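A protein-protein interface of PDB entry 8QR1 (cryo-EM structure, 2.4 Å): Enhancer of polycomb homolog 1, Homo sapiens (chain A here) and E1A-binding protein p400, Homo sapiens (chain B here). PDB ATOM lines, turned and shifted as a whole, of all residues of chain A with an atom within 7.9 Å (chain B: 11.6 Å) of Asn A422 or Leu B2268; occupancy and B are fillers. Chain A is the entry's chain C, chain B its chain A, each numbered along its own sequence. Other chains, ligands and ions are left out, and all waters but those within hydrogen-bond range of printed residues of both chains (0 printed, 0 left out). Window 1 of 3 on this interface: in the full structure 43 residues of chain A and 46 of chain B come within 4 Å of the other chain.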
ATOM      1  N   PRO A 415      16.544  20.000 -14.767  1.00  0.00           N
ATOM      2  CA  PRO A 415      16.863  19.809 -16.185  1.00  0.00           C
ATOM      3  C   PRO A 415      18.343  19.993 -16.471  1.00  0.00           C
ATOM      4  O   PRO A 415      19.084  20.590 -15.687  1.00  0.00           O
ATOM      5  CB  PRO A 415      16.034  20.891 -16.875  1.00  0.00           C
ATOM      6  CG  PRO A 415      15.976  21.965 -15.899  1.00  0.00           C
ATOM      7  CD  PRO A 415      15.967  21.338 -14.541  1.00  0.00           C
ATOM      8  N   HIS A 416      18.767  19.469 -17.618  1.00  0.00           N
ATOM      9  CA  HIS A 416      20.120  19.689 -18.127  1.00  0.00           C
ATOM     10  C   HIS A 416      20.171  21.032 -18.843  1.00  0.00           C
ATOM     11  O   HIS A 416      19.637  21.182 -19.943  1.00  0.00           O
ATOM     12  CB  HIS A 416      20.535  18.567 -19.069  1.00  0.00           C
ATOM     13  CG  HIS A 416      20.674  17.233 -18.410  1.00  0.00           C
ATOM     14  ND1 HIS A 416      21.384  17.052 -17.245  1.00  0.00           N
ATOM     15  CD2 HIS A 416      20.234  16.007 -18.777  1.00  0.00           C
ATOM     16  CE1 HIS A 416      21.356  15.775 -16.908  1.00  0.00           C
ATOM     17  NE2 HIS A 416      20.664  15.119 -17.821  1.00  0.00           N
ATOM     18  N   GLN A 419      24.770  21.205 -20.622  1.00  0.00           N
ATOM     19  CA  GLN A 419      25.135  20.294 -21.697  1.00  0.00           C
ATOM     20  C   GLN A 419      23.981  19.342 -21.951  1.00  0.00           C
ATOM     21  O   GLN A 419      23.342  18.867 -21.011  1.00  0.00           O
ATOM     22  CB  GLN A 419      26.402  19.506 -21.349  1.00  0.00           C
ATOM     23  CG  GLN A 419      26.824  18.481 -22.399  1.00  0.00           C
ATOM     24  CD  GLN A 419      28.235  17.954 -22.195  1.00  0.00           C
ATOM     25  OE1 GLN A 419      28.992  17.804 -23.152  1.00  0.00           O
ATOM     26  NE2 GLN A 419      28.587  17.644 -20.951  1.00  0.00           N
ATOM     27  N   THR A 420      23.727  19.062 -23.225  1.00  0.00           N
ATOM     28  CA  THR A 420      22.660  18.146 -23.593  1.00  0.00           C
ATOM     29  C   THR A 420      22.967  16.741 -23.091  1.00  0.00           C
ATOM     30  O   THR A 420      24.126  16.320 -23.053  1.00  0.00           O
ATOM     31  CB  THR A 420      22.477  18.134 -25.107  1.00  0.00           C
ATOM     32  OG1 THR A 420      22.701  19.449 -25.630  1.00  0.00           O
ATOM     33  CG2 THR A 420      21.079  17.679 -25.466  1.00  0.00           C
ATOM     34  N   GLY A 421      21.922  16.021 -22.704  1.00  0.00           N
ATOM     35  CA  GLY A 421      22.089  14.676 -22.202  1.00  0.00           C
ATOM     36  C   GLY A 421      22.363  13.681 -23.310  1.00  0.00           C
ATOM     37  O   GLY A 421      22.339  13.991 -24.501  1.00  0.00           O
ATOM     38  N   ASN A 422      22.635  12.449 -22.894  1.00  0.00           N
ATOM     39  CA  ASN A 422      22.943  11.376 -23.827  1.00  0.00           C
ATOM     40  C   ASN A 422      22.653  10.049 -23.144  1.00  0.00           C
ATOM     41  O   ASN A 422      22.332   9.994 -21.955  1.00  0.00           O
ATOM     42  CB  ASN A 422      24.395  11.451 -24.305  1.00  0.00           C
ATOM     43  CG  ASN A 422      24.589  10.899 -25.699  1.00  0.00           C
ATOM     44  OD1 ASN A 422      23.760  10.149 -26.211  1.00  0.00           O
ATOM     45  ND2 ASN A 422      25.697  11.269 -26.320  1.00  0.00           N
ATOM     46  N   TRP A 423      22.768   8.976 -23.920  1.00  0.00           N
ATOM     47  CA  TRP A 423      22.421   7.654 -23.444  1.00  0.00           C
ATOM     48  C   TRP A 423      23.422   7.179 -22.392  1.00  0.00           C
ATOM     49  O   TRP A 423      24.435   7.836 -22.148  1.00  0.00           O
ATOM     50  CB  TRP A 423      22.383   6.681 -24.617  1.00  0.00           C
ATOM     51  CG  TRP A 423      21.387   7.038 -25.658  1.00  0.00           C
ATOM     52  CD1 TRP A 423      21.622   7.698 -26.822  1.00  0.00           C
ATOM     53  CD2 TRP A 423      19.988   6.748 -25.635  1.00  0.00           C
ATOM     54  NE1 TRP A 423      20.456   7.842 -27.527  1.00  0.00           N
ATOM     55  CE2 TRP A 423      19.437   7.266 -26.819  1.00  0.00           C
ATOM     56  CE3 TRP A 423      19.147   6.102 -24.727  1.00  0.00           C
ATOM     57  CZ2 TRP A 423      18.087   7.157 -27.118  1.00  0.00           C
ATOM     58  CZ3 TRP A 423      17.808   5.997 -25.027  1.00  0.00           C
ATOM     59  CH2 TRP A 423      17.291   6.521 -26.210  1.00  0.00           C
ATOM     60  N   PRO A 424      23.161   6.038 -21.744  1.00  0.00           N
ATOM     61  CA  PRO A 424      24.187   5.444 -20.873  1.00  0.00           C
ATOM     62  C   PRO A 424      25.390   4.877 -21.615  1.00  0.00           C
ATOM     63  O   PRO A 424      26.389   4.554 -20.961  1.00  0.00           O
ATOM     64  CB  PRO A 424      23.427   4.335 -20.137  1.00  0.00           C
ATOM     65  CG  PRO A 424      22.018   4.691 -20.249  1.00  0.00           C
ATOM     66  CD  PRO A 424      21.862   5.369 -21.559  1.00  0.00           C
ATOM     67  N   TRP A 425      25.328   4.754 -22.941  1.00  0.00           N
ATOM     68  CA  TRP A 425      26.334   4.072 -23.742  1.00  0.00           C
ATOM     69  C   TRP A 425      26.644   4.924 -24.961  1.00  0.00           C
ATOM     70  O   TRP A 425      25.857   5.788 -25.355  1.00  0.00           O
ATOM     71  CB  TRP A 425      25.858   2.684 -24.168  1.00  0.00           C
ATOM     72  CG  TRP A 425      24.379   2.579 -24.269  1.00  0.00           C
ATOM     73  CD1 TRP A 425      23.537   1.976 -23.386  1.00  0.00           C
ATOM     74  CD2 TRP A 425      23.558   3.112 -25.308  1.00  0.00           C
ATOM     75  NE1 TRP A 425      22.239   2.095 -23.815  1.00  0.00           N
ATOM     76  CE2 TRP A 425      22.226   2.788 -24.995  1.00  0.00           C
ATOM     77  CE3 TRP A 425      23.821   3.827 -26.477  1.00  0.00           C
ATOM     78  CZ2 TRP A 425      21.163   3.154 -25.803  1.00  0.00           C
ATOM     79  CZ3 TRP A 425      22.765   4.190 -27.278  1.00  0.00           C
ATOM     80  CH2 TRP A 425      21.450   3.853 -26.940  1.00  0.00           C
ATOM     81  N   THR A 426      27.820   4.695 -25.543  1.00  0.00           N
ATOM     82  CA  THR A 426      28.415   5.578 -26.545  1.00  0.00           C
ATOM     83  C   THR A 426      28.592   6.995 -26.013  1.00  0.00           C
ATOM     84  O   THR A 426      28.605   7.951 -26.798  1.00  0.00           O
ATOM     85  CB  THR A 426      27.593   5.625 -27.849  1.00  0.00           C
ATOM     86  OG1 THR A 426      26.338   6.280 -27.616  1.00  0.00           O
ATOM     87  CG2 THR A 426      27.340   4.231 -28.426  1.00  0.00           C
ATOM     88  N   SER A 427      28.736   7.149 -24.694  1.00  0.00           N
ATOM     89  CA  SER A 427      28.507   8.423 -24.018  1.00  0.00           C
ATOM     90  C   SER A 427      29.315   8.435 -22.726  1.00  0.00           C
ATOM     91  O   SER A 427      28.879   7.866 -21.712  1.00  0.00           O
ATOM     92  CB  SER A 427      27.023   8.616 -23.727  1.00  0.00           C
ATOM     93  OG  SER A 427      26.253   8.519 -24.908  1.00  0.00           O
ATOM     94  N   PRO A 428      30.496   9.054 -22.713  1.00  0.00           N
ATOM     95  CA  PRO A 428      31.177   9.289 -21.436  1.00  0.00           C
ATOM     96  C   PRO A 428      30.462  10.356 -20.621  1.00  0.00           C
ATOM     97  O   PRO A 428      29.414  10.880 -21.001  1.00  0.00           O
ATOM     98  CB  PRO A 428      32.585   9.729 -21.858  1.00  0.00           C
ATOM     99  CG  PRO A 428      32.446  10.205 -23.227  1.00  0.00           C
ATOM    100  CD  PRO A 428      31.383   9.373 -23.849  1.00  0.00           C
ATOM    101  N   ASP A 430      31.466  13.235 -20.424  1.00  0.00           N
ATOM    102  CA  ASP A 430      31.412  14.352 -21.355  1.00  0.00           C
ATOM    103  C   ASP A 430      30.272  14.163 -22.354  1.00  0.00           C
ATOM    104  O   ASP A 430      30.516  14.000 -23.554  1.00  0.00           O
ATOM    105  CB  ASP A 430      32.746  14.496 -22.088  1.00  0.00           C
ATOM    106  CG  ASP A 430      33.932  14.498 -21.145  1.00  0.00           C
ATOM    107  OD1 ASP A 430      35.064  14.745 -21.612  1.00  0.00           O
ATOM    108  OD2 ASP A 430      33.733  14.242 -19.939  1.00  0.00           O
ATOM    109  N   GLY A 431      29.029  14.202 -21.866  1.00  0.00           N
ATOM    110  CA  GLY A 431      27.846  14.069 -22.697  1.00  0.00           C
ATOM    111  C   GLY A 431      26.704  13.291 -22.074  1.00  0.00           C
ATOM    112  O   GLY A 431      25.542  13.624 -22.311  1.00  0.00           O
ATOM    113  N   GLY A 432      27.001  12.282 -21.259  1.00  0.00           N
ATOM    114  CA  GLY A 432      25.949  11.440 -20.718  1.00  0.00           C
ATOM    115  C   GLY A 432      26.384  10.526 -19.593  1.00  0.00           C
ATOM    116  O   GLY A 432      27.470  10.686 -19.042  1.00  0.00           O
ATOM    117  N   LEU A 433      25.542   9.561 -19.240  1.00  0.00           N
ATOM    118  CA  LEU A 433      25.851   8.664 -18.133  1.00  0.00           C
ATOM    119  C   LEU A 433      26.900   7.648 -18.569  1.00  0.00           C
ATOM    120  O   LEU A 433      26.728   6.963 -19.581  1.00  0.00           O
ATOM    121  CB  LEU A 433      24.578   7.967 -17.655  1.00  0.00           C
ATOM    122  CG  LEU A 433      24.681   6.914 -16.546  1.00  0.00           C
ATOM    123  CD1 LEU A 433      25.210   7.530 -15.275  1.00  0.00           C
ATOM    124  CD2 LEU A 433      23.328   6.272 -16.301  1.00  0.00           C
ATOM    125  N   GLY A 434      27.991   7.568 -17.813  1.00  0.00           N
ATOM    126  CA  GLY A 434      29.045   6.607 -18.066  1.00  0.00           C
ATOM    127  C   GLY A 434      28.905   5.333 -17.264  1.00  0.00           C
ATOM    128  O   GLY A 434      29.684   5.101 -16.335  1.00  0.00           O
ATOM    129  N   ARG B 798      13.732  26.372 -17.793  1.00  0.00           N
ATOM    130  CA  ARG B 798      12.854  25.224 -17.968  1.00  0.00           C
ATOM    131  C   ARG B 798      12.368  24.706 -16.624  1.00  0.00           C
ATOM    132  O   ARG B 798      13.097  24.730 -15.630  1.00  0.00           O
ATOM    133  CB  ARG B 798      13.571  24.095 -18.708  1.00  0.00           C
ATOM    134  CG  ARG B 798      13.438  24.137 -20.207  1.00  0.00           C
ATOM    135  CD  ARG B 798      14.176  22.978 -20.840  1.00  0.00           C
ATOM    136  NE  ARG B 798      15.616  23.205 -20.870  1.00  0.00           N
ATOM    137  CZ  ARG B 798      16.556  22.265 -20.868  1.00  0.00           C
ATOM    138  NH1 ARG B 798      16.262  20.972 -20.818  1.00  0.00           N
ATOM    139  NH2 ARG B 798      17.832  22.631 -20.924  1.00  0.00           N
ATOM    140  N   LEU B 799      11.128  24.232 -16.605  1.00  0.00           N
ATOM    141  CA  LEU B 799      10.581  23.658 -15.395  1.00  0.00           C
ATOM    142  C   LEU B 799      11.171  22.263 -15.171  1.00  0.00           C
ATOM    143  O   LEU B 799      11.574  21.599 -16.129  1.00  0.00           O
ATOM    144  CB  LEU B 799       9.064  23.561 -15.487  1.00  0.00           C
ATOM    145  CG  LEU B 799       8.257  24.843 -15.318  1.00  0.00           C
ATOM    146  CD1 LEU B 799       6.855  24.609 -15.811  1.00  0.00           C
ATOM    147  CD2 LEU B 799       8.240  25.296 -13.881  1.00  0.00           C
ATOM    148  N   LYS B 801      11.174  18.136 -13.991  1.00  0.00           N
ATOM    149  CA  LYS B 801      10.291  16.993 -14.171  1.00  0.00           C
ATOM    150  C   LYS B 801       9.800  16.492 -12.820  1.00  0.00           C
ATOM    151  O   LYS B 801      10.598  16.186 -11.930  1.00  0.00           O
ATOM    152  CB  LYS B 801      11.032  15.881 -14.912  1.00  0.00           C
ATOM    153  CG  LYS B 801      10.190  15.021 -15.843  1.00  0.00           C
ATOM    154  CD  LYS B 801       9.159  14.218 -15.106  1.00  0.00           C
ATOM    155  CE  LYS B 801       8.514  13.183 -15.986  1.00  0.00           C
ATOM    156  NZ  LYS B 801       7.260  12.682 -15.367  1.00  0.00           N
ATOM    157  N   GLN B 820      19.767  -6.300 -25.130  1.00  0.00           N
ATOM    158  CA  GLN B 820      20.971  -5.505 -25.366  1.00  0.00           C
ATOM    159  C   GLN B 820      22.214  -6.382 -25.310  1.00  0.00           C
ATOM    160  O   GLN B 820      23.085  -6.322 -26.194  1.00  0.00           O
ATOM    161  CB  GLN B 820      21.072  -4.393 -24.325  1.00  0.00           C
ATOM    162  CG  GLN B 820      20.033  -3.310 -24.438  1.00  0.00           C
ATOM    163  CD  GLN B 820      20.578  -1.946 -24.069  1.00  0.00           C
ATOM    164  OE1 GLN B 820      21.146  -1.766 -22.993  1.00  0.00           O
ATOM    165  NE2 GLN B 820      20.384  -0.971 -24.948  1.00  0.00           N
ATOM    166  N   LEU B2262      14.493   2.682 -14.111  1.00  0.00           N
ATOM    167  CA  LEU B2262      14.946   4.017 -14.471  1.00  0.00           C
ATOM    168  C   LEU B2262      14.631   4.252 -15.938  1.00  0.00           C
ATOM    169  O   LEU B2262      14.988   3.434 -16.791  1.00  0.00           O
ATOM    170  CB  LEU B2262      16.448   4.175 -14.212  1.00  0.00           C
ATOM    171  CG  LEU B2262      17.114   5.511 -14.558  1.00  0.00           C
ATOM    172  CD1 LEU B2262      16.501   6.664 -13.781  1.00  0.00           C
ATOM    173  CD2 LEU B2262      18.601   5.417 -14.285  1.00  0.00           C
ATOM    174  N   ASP B2263      13.968   5.368 -16.226  1.00  0.00           N
ATOM    175  CA  ASP B2263      13.635   5.742 -17.598  1.00  0.00           C
ATOM    176  C   ASP B2263      14.854   6.418 -18.210  1.00  0.00           C
ATOM    177  O   ASP B2263      15.165   7.570 -17.900  1.00  0.00           O
ATOM    178  CB  ASP B2263      12.415   6.653 -17.623  1.00  0.00           C
ATOM    179  CG  ASP B2263      11.748   6.702 -18.983  1.00  0.00           C
ATOM    180  OD1 ASP B2263      12.416   6.387 -19.989  1.00  0.00           O
ATOM    181  OD2 ASP B2263      10.553   7.057 -19.046  1.00  0.00           O
ATOM    182  N   SER B2264      15.557   5.694 -19.081  1.00  0.00           N
ATOM    183  CA  SER B2264      16.754   6.237 -19.707  1.00  0.00           C
ATOM    184  C   SER B2264      16.441   7.380 -20.658  1.00  0.00           C
ATOM    185  O   SER B2264      17.280   8.269 -20.836  1.00  0.00           O
ATOM    186  CB  SER B2264      17.498   5.133 -20.453  1.00  0.00           C
ATOM    187  OG  SER B2264      17.821   4.062 -19.585  1.00  0.00           O
ATOM    188  N   VAL B2265      15.263   7.372 -21.278  1.00  0.00           N
ATOM    189  CA  VAL B2265      14.896   8.444 -22.196  1.00  0.00           C
ATOM    190  C   VAL B2265      14.683   9.747 -21.440  1.00  0.00           C
ATOM    191  O   VAL B2265      15.020  10.827 -21.936  1.00  0.00           O
ATOM    192  CB  VAL B2265      13.649   8.048 -23.004  1.00  0.00           C
ATOM    193  CG1 VAL B2265      13.221   9.194 -23.904  1.00  0.00           C
ATOM    194  CG2 VAL B2265      13.921   6.788 -23.816  1.00  0.00           C
ATOM    195  N   MET B2266      14.113   9.673 -20.237  1.00  0.00           N
ATOM    196  CA  MET B2266      13.906  10.882 -19.449  1.00  0.00           C
ATOM    197  C   MET B2266      15.225  11.468 -18.969  1.00  0.00           C
ATOM    198  O   MET B2266      15.319  12.680 -18.745  1.00  0.00           O
ATOM    199  CB  MET B2266      12.997  10.587 -18.257  1.00  0.00           C
ATOM    200  CG  MET B2266      12.058  11.730 -17.886  1.00  0.00           C
ATOM    201  SD  MET B2266      10.770  12.162 -19.086  1.00  0.00           S
ATOM    202  CE  MET B2266      10.001  10.584 -19.442  1.00  0.00           C
ATOM    203  N   CYS B2267      16.253  10.634 -18.807  1.00  0.00           N
ATOM    204  CA  CYS B2267      17.567  11.126 -18.419  1.00  0.00           C
ATOM    205  C   CYS B2267      18.252  11.931 -19.516  1.00  0.00           C
ATOM    206  O   CYS B2267      19.243  12.610 -19.231  1.00  0.00           O
ATOM    207  CB  CYS B2267      18.458   9.956 -18.007  1.00  0.00           C
ATOM    208  SG  CYS B2267      18.023   9.220 -16.420  1.00  0.00           S
ATOM    209  N   LEU B2268      17.764  11.867 -20.756  1.00  0.00           N
ATOM    210  CA  LEU B2268      18.318  12.690 -21.823  1.00  0.00           C
ATOM    211  C   LEU B2268      18.053  14.174 -21.614  1.00  0.00           C
ATOM    212  O   LEU B2268      18.808  14.997 -22.142  1.00  0.00           O
ATOM    213  CB  LEU B2268      17.736  12.260 -23.167  1.00  0.00           C
ATOM    214  CG  LEU B2268      17.944  10.807 -23.591  1.00  0.00           C
ATOM    215  CD1 LEU B2268      17.108  10.489 -24.801  1.00  0.00           C
ATOM    216  CD2 LEU B2268      19.391  10.538 -23.883  1.00  0.00           C
ATOM    217  N   MET B2269      17.004  14.526 -20.862  1.00  0.00           N
ATOM    218  CA  MET B2269      16.600  15.905 -20.626  1.00  0.00           C
ATOM    219  C   MET B2269      16.684  16.342 -19.174  1.00  0.00           C
ATOM    220  O   MET B2269      16.716  17.551 -18.924  1.00  0.00           O
ATOM    221  CB  MET B2269      15.156  16.121 -21.099  1.00  0.00           C
ATOM    222  CG  MET B2269      14.991  16.231 -22.593  1.00  0.00           C
ATOM    223  SD  MET B2269      15.159  17.919 -23.192  1.00  0.00           S
ATOM    224  CE  MET B2269      16.761  17.823 -23.974  1.00  0.00           C
ATOM    225  N   TYR B2270      16.717  15.410 -18.220  1.00  0.00           N
ATOM    226  CA  TYR B2270      16.617  15.718 -16.801  1.00  0.00           C
ATOM    227  C   TYR B2270      17.613  14.883 -16.011  1.00  0.00           C
ATOM    228  O   TYR B2270      18.054  13.823 -16.456  1.00  0.00           O
ATOM    229  CB  TYR B2270      15.197  15.471 -16.286  1.00  0.00           C
ATOM    230  CG  TYR B2270      14.163  16.328 -16.971  1.00  0.00           C
ATOM    231  CD1 TYR B2270      14.001  17.656 -16.625  1.00  0.00           C
ATOM    232  CD2 TYR B2270      13.355  15.811 -17.969  1.00  0.00           C
ATOM    233  CE1 TYR B2270      13.067  18.444 -17.251  1.00  0.00           C
ATOM    234  CE2 TYR B2270      12.416  16.592 -18.598  1.00  0.00           C
ATOM    235  CZ  TYR B2270      12.277  17.909 -18.235  1.00  0.00           C
ATOM    236  OH  TYR B2270      11.345  18.702 -18.854  1.00  0.00           O
ATOM    237  N   GLU B2271      17.968  15.386 -14.833  1.00  0.00           N
ATOM    238  CA  GLU B2271      18.942  14.710 -13.989  1.00  0.00           C
ATOM    239  C   GLU B2271      18.381  13.393 -13.467  1.00  0.00           C
ATOM    240  O   GLU B2271      17.168  13.203 -13.357  1.00  0.00           O
ATOM    241  CB  GLU B2271      19.345  15.606 -12.821  1.00  0.00           C
ATOM    242  CG  GLU B2271      20.137  16.845 -13.221  1.00  0.00           C
ATOM    243  CD  GLU B2271      21.605  16.560 -13.465  1.00  0.00           C
ATOM    244  OE1 GLU B2271      21.968  15.379 -13.646  1.00  0.00           O
ATOM    245  OE2 GLU B2271      22.400  17.523 -13.478  1.00  0.00           O
ATOM    246  N   ALA B2272      19.291  12.473 -13.142  1.00  0.00           N
ATOM    247  CA  ALA B2272      18.894  11.138 -12.716  1.00  0.00           C
ATOM    248  C   ALA B2272      18.335  11.106 -11.301  1.00  0.00           C
ATOM    249  O   ALA B2272      17.506  10.239 -11.005  1.00  0.00           O
ATOM    250  CB  ALA B2272      20.086  10.188 -12.813  1.00  0.00           C
ATOM    251  N   THR B2273      18.759  12.026 -10.434  1.00  0.00           N
ATOM    252  CA  THR B2273      18.390  12.078  -9.028  1.00  0.00           C
ATOM    253  C   THR B2273      17.564  13.329  -8.760  1.00  0.00           C
ATOM    254  O   THR B2273      17.722  14.332  -9.462  1.00  0.00           O
ATOM    255  CB  THR B2273      19.637  12.093  -8.134  1.00  0.00           C
ATOM    256  OG1 THR B2273      20.519  13.138  -8.562  1.00  0.00           O
ATOM    257  CG2 THR B2273      20.358  10.759  -8.200  1.00  0.00           C
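NH2 of Arg B798 is in hydrogen-bond range of O of His A416, 2.5 Å away. NE2 of His A416 is in hydrogen-bond range of O of Cys B2267, 3.2 Å away. The backbone carbonyl oxygen (O) of Leu B2268 sits close to the backbone NH (N) of Gly A421 (3.3 Å). N of His A416 lies within hydrogen-bond range of O of Met B2269 (3.1 Å). A ring nitrogen (NE2) of His A416 sits at hydrogen-bond distance from the backbone carbonyl oxygen of Tyr B2270 (3.2 Å).
The backbone carbonyl oxygen (O) of Asp B2263 sits at hydrogen-bond distance from the side-chain sulfur (SG) of Cys B2267 (3.6 Å). The side-chain amide nitrogen (ND2) of Asn A422 sits close to the side-chain hydroxyl (OG) of Ser A427 (3.1 Å). N of Asn A422 sits close to O of Gly A431, 3.2 Å away. The backbone carbonyl oxygen of Trp A423 lies close to the side-chain hydroxyl of Ser A427 (3.4 Å). The side-chain hydroxyl (OG) of Ser A427 lies within hydrogen-bond range of the backbone carbonyl oxygen (O) of Trp A425 (2.8 Å).
NH1 of Arg B798 touches CB of Pro A415, 3.95 Å away. O of Met B2269 touches CA of Pro A415, at 3.6 Å. Pro A415 touches Tyr B2270 (CA to CD1, 3.6 Å). CD2 of His A416 touches O of Leu B2268, 3.8 Å away. CE1 of His A416 touches OE1 of Glu B2271, 3.3 Å away. C of Asn A422 touches CD2 of Leu B2268, at 3.4 Å. Leu B2268 touches Trp A423 (CD2 to N, 3.7 Å). Gln B820 touches Trp A425.
Of the printed residues of chain B, Pro A415 touches Arg B798 (3.95 Å), Met B2269 (3.6 Å) and Tyr B2270 (3.6 Å). Of chain B, only Arg B798 (2.5 Å), Cys B2267 (3.2 Å), Leu B2268 (3.8 Å), Met B2269 (3.1 Å), Tyr B2270 (3.2 Å) and Glu B2271 (3.3 Å) come within 4 Å of His A416. No residue of chain B comes within 4 Å of Thr A420. Asn A422 touches just one residue of chain B: Leu B2268 (3.4 Å). Trp A423 touches one residue of chain B. Pro A424 touches none of the printed residues of chain B. Of the printed residues of chain B, Trp A425 touches Gln B820. No residue of chain B comes within 4 Å of Thr A426. No residue of chain B comes within 4 Å of Ser A427. Gly A431 touches none of the printed residues of chain B. Leu A433 touches none of the printed residues of chain B. Of the printed residues of chain A, Arg B798 touches Pro A415 and His A416. Leu B2268 touches four residues of chain A. Of the printed residues of chain A, Tyr B2270 touches Pro A415 and His A416. Of the printed residues of chain A, Glu B2271 touches His A416. Ala B2272 touches none of the printed residues of chain A. The nearest residue of chain B that does not touch Asn A422 is Cys B2267 (4.9 Å). The nearest printed residue of chain A that does not touch Arg B798 is Gln A419 (6.7 Å).
Hydrophobic or aromatic side chains of chain B within 4 Å of the printed part of chain A: Leu B2268 and Tyr B2270. Among the printed residues, 13 pairs touch across the chains. Among the printed residues, no Asp or Glu carboxylate lies within 4 Å of a Lys or Arg side-chain nitrogen of the other chain.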
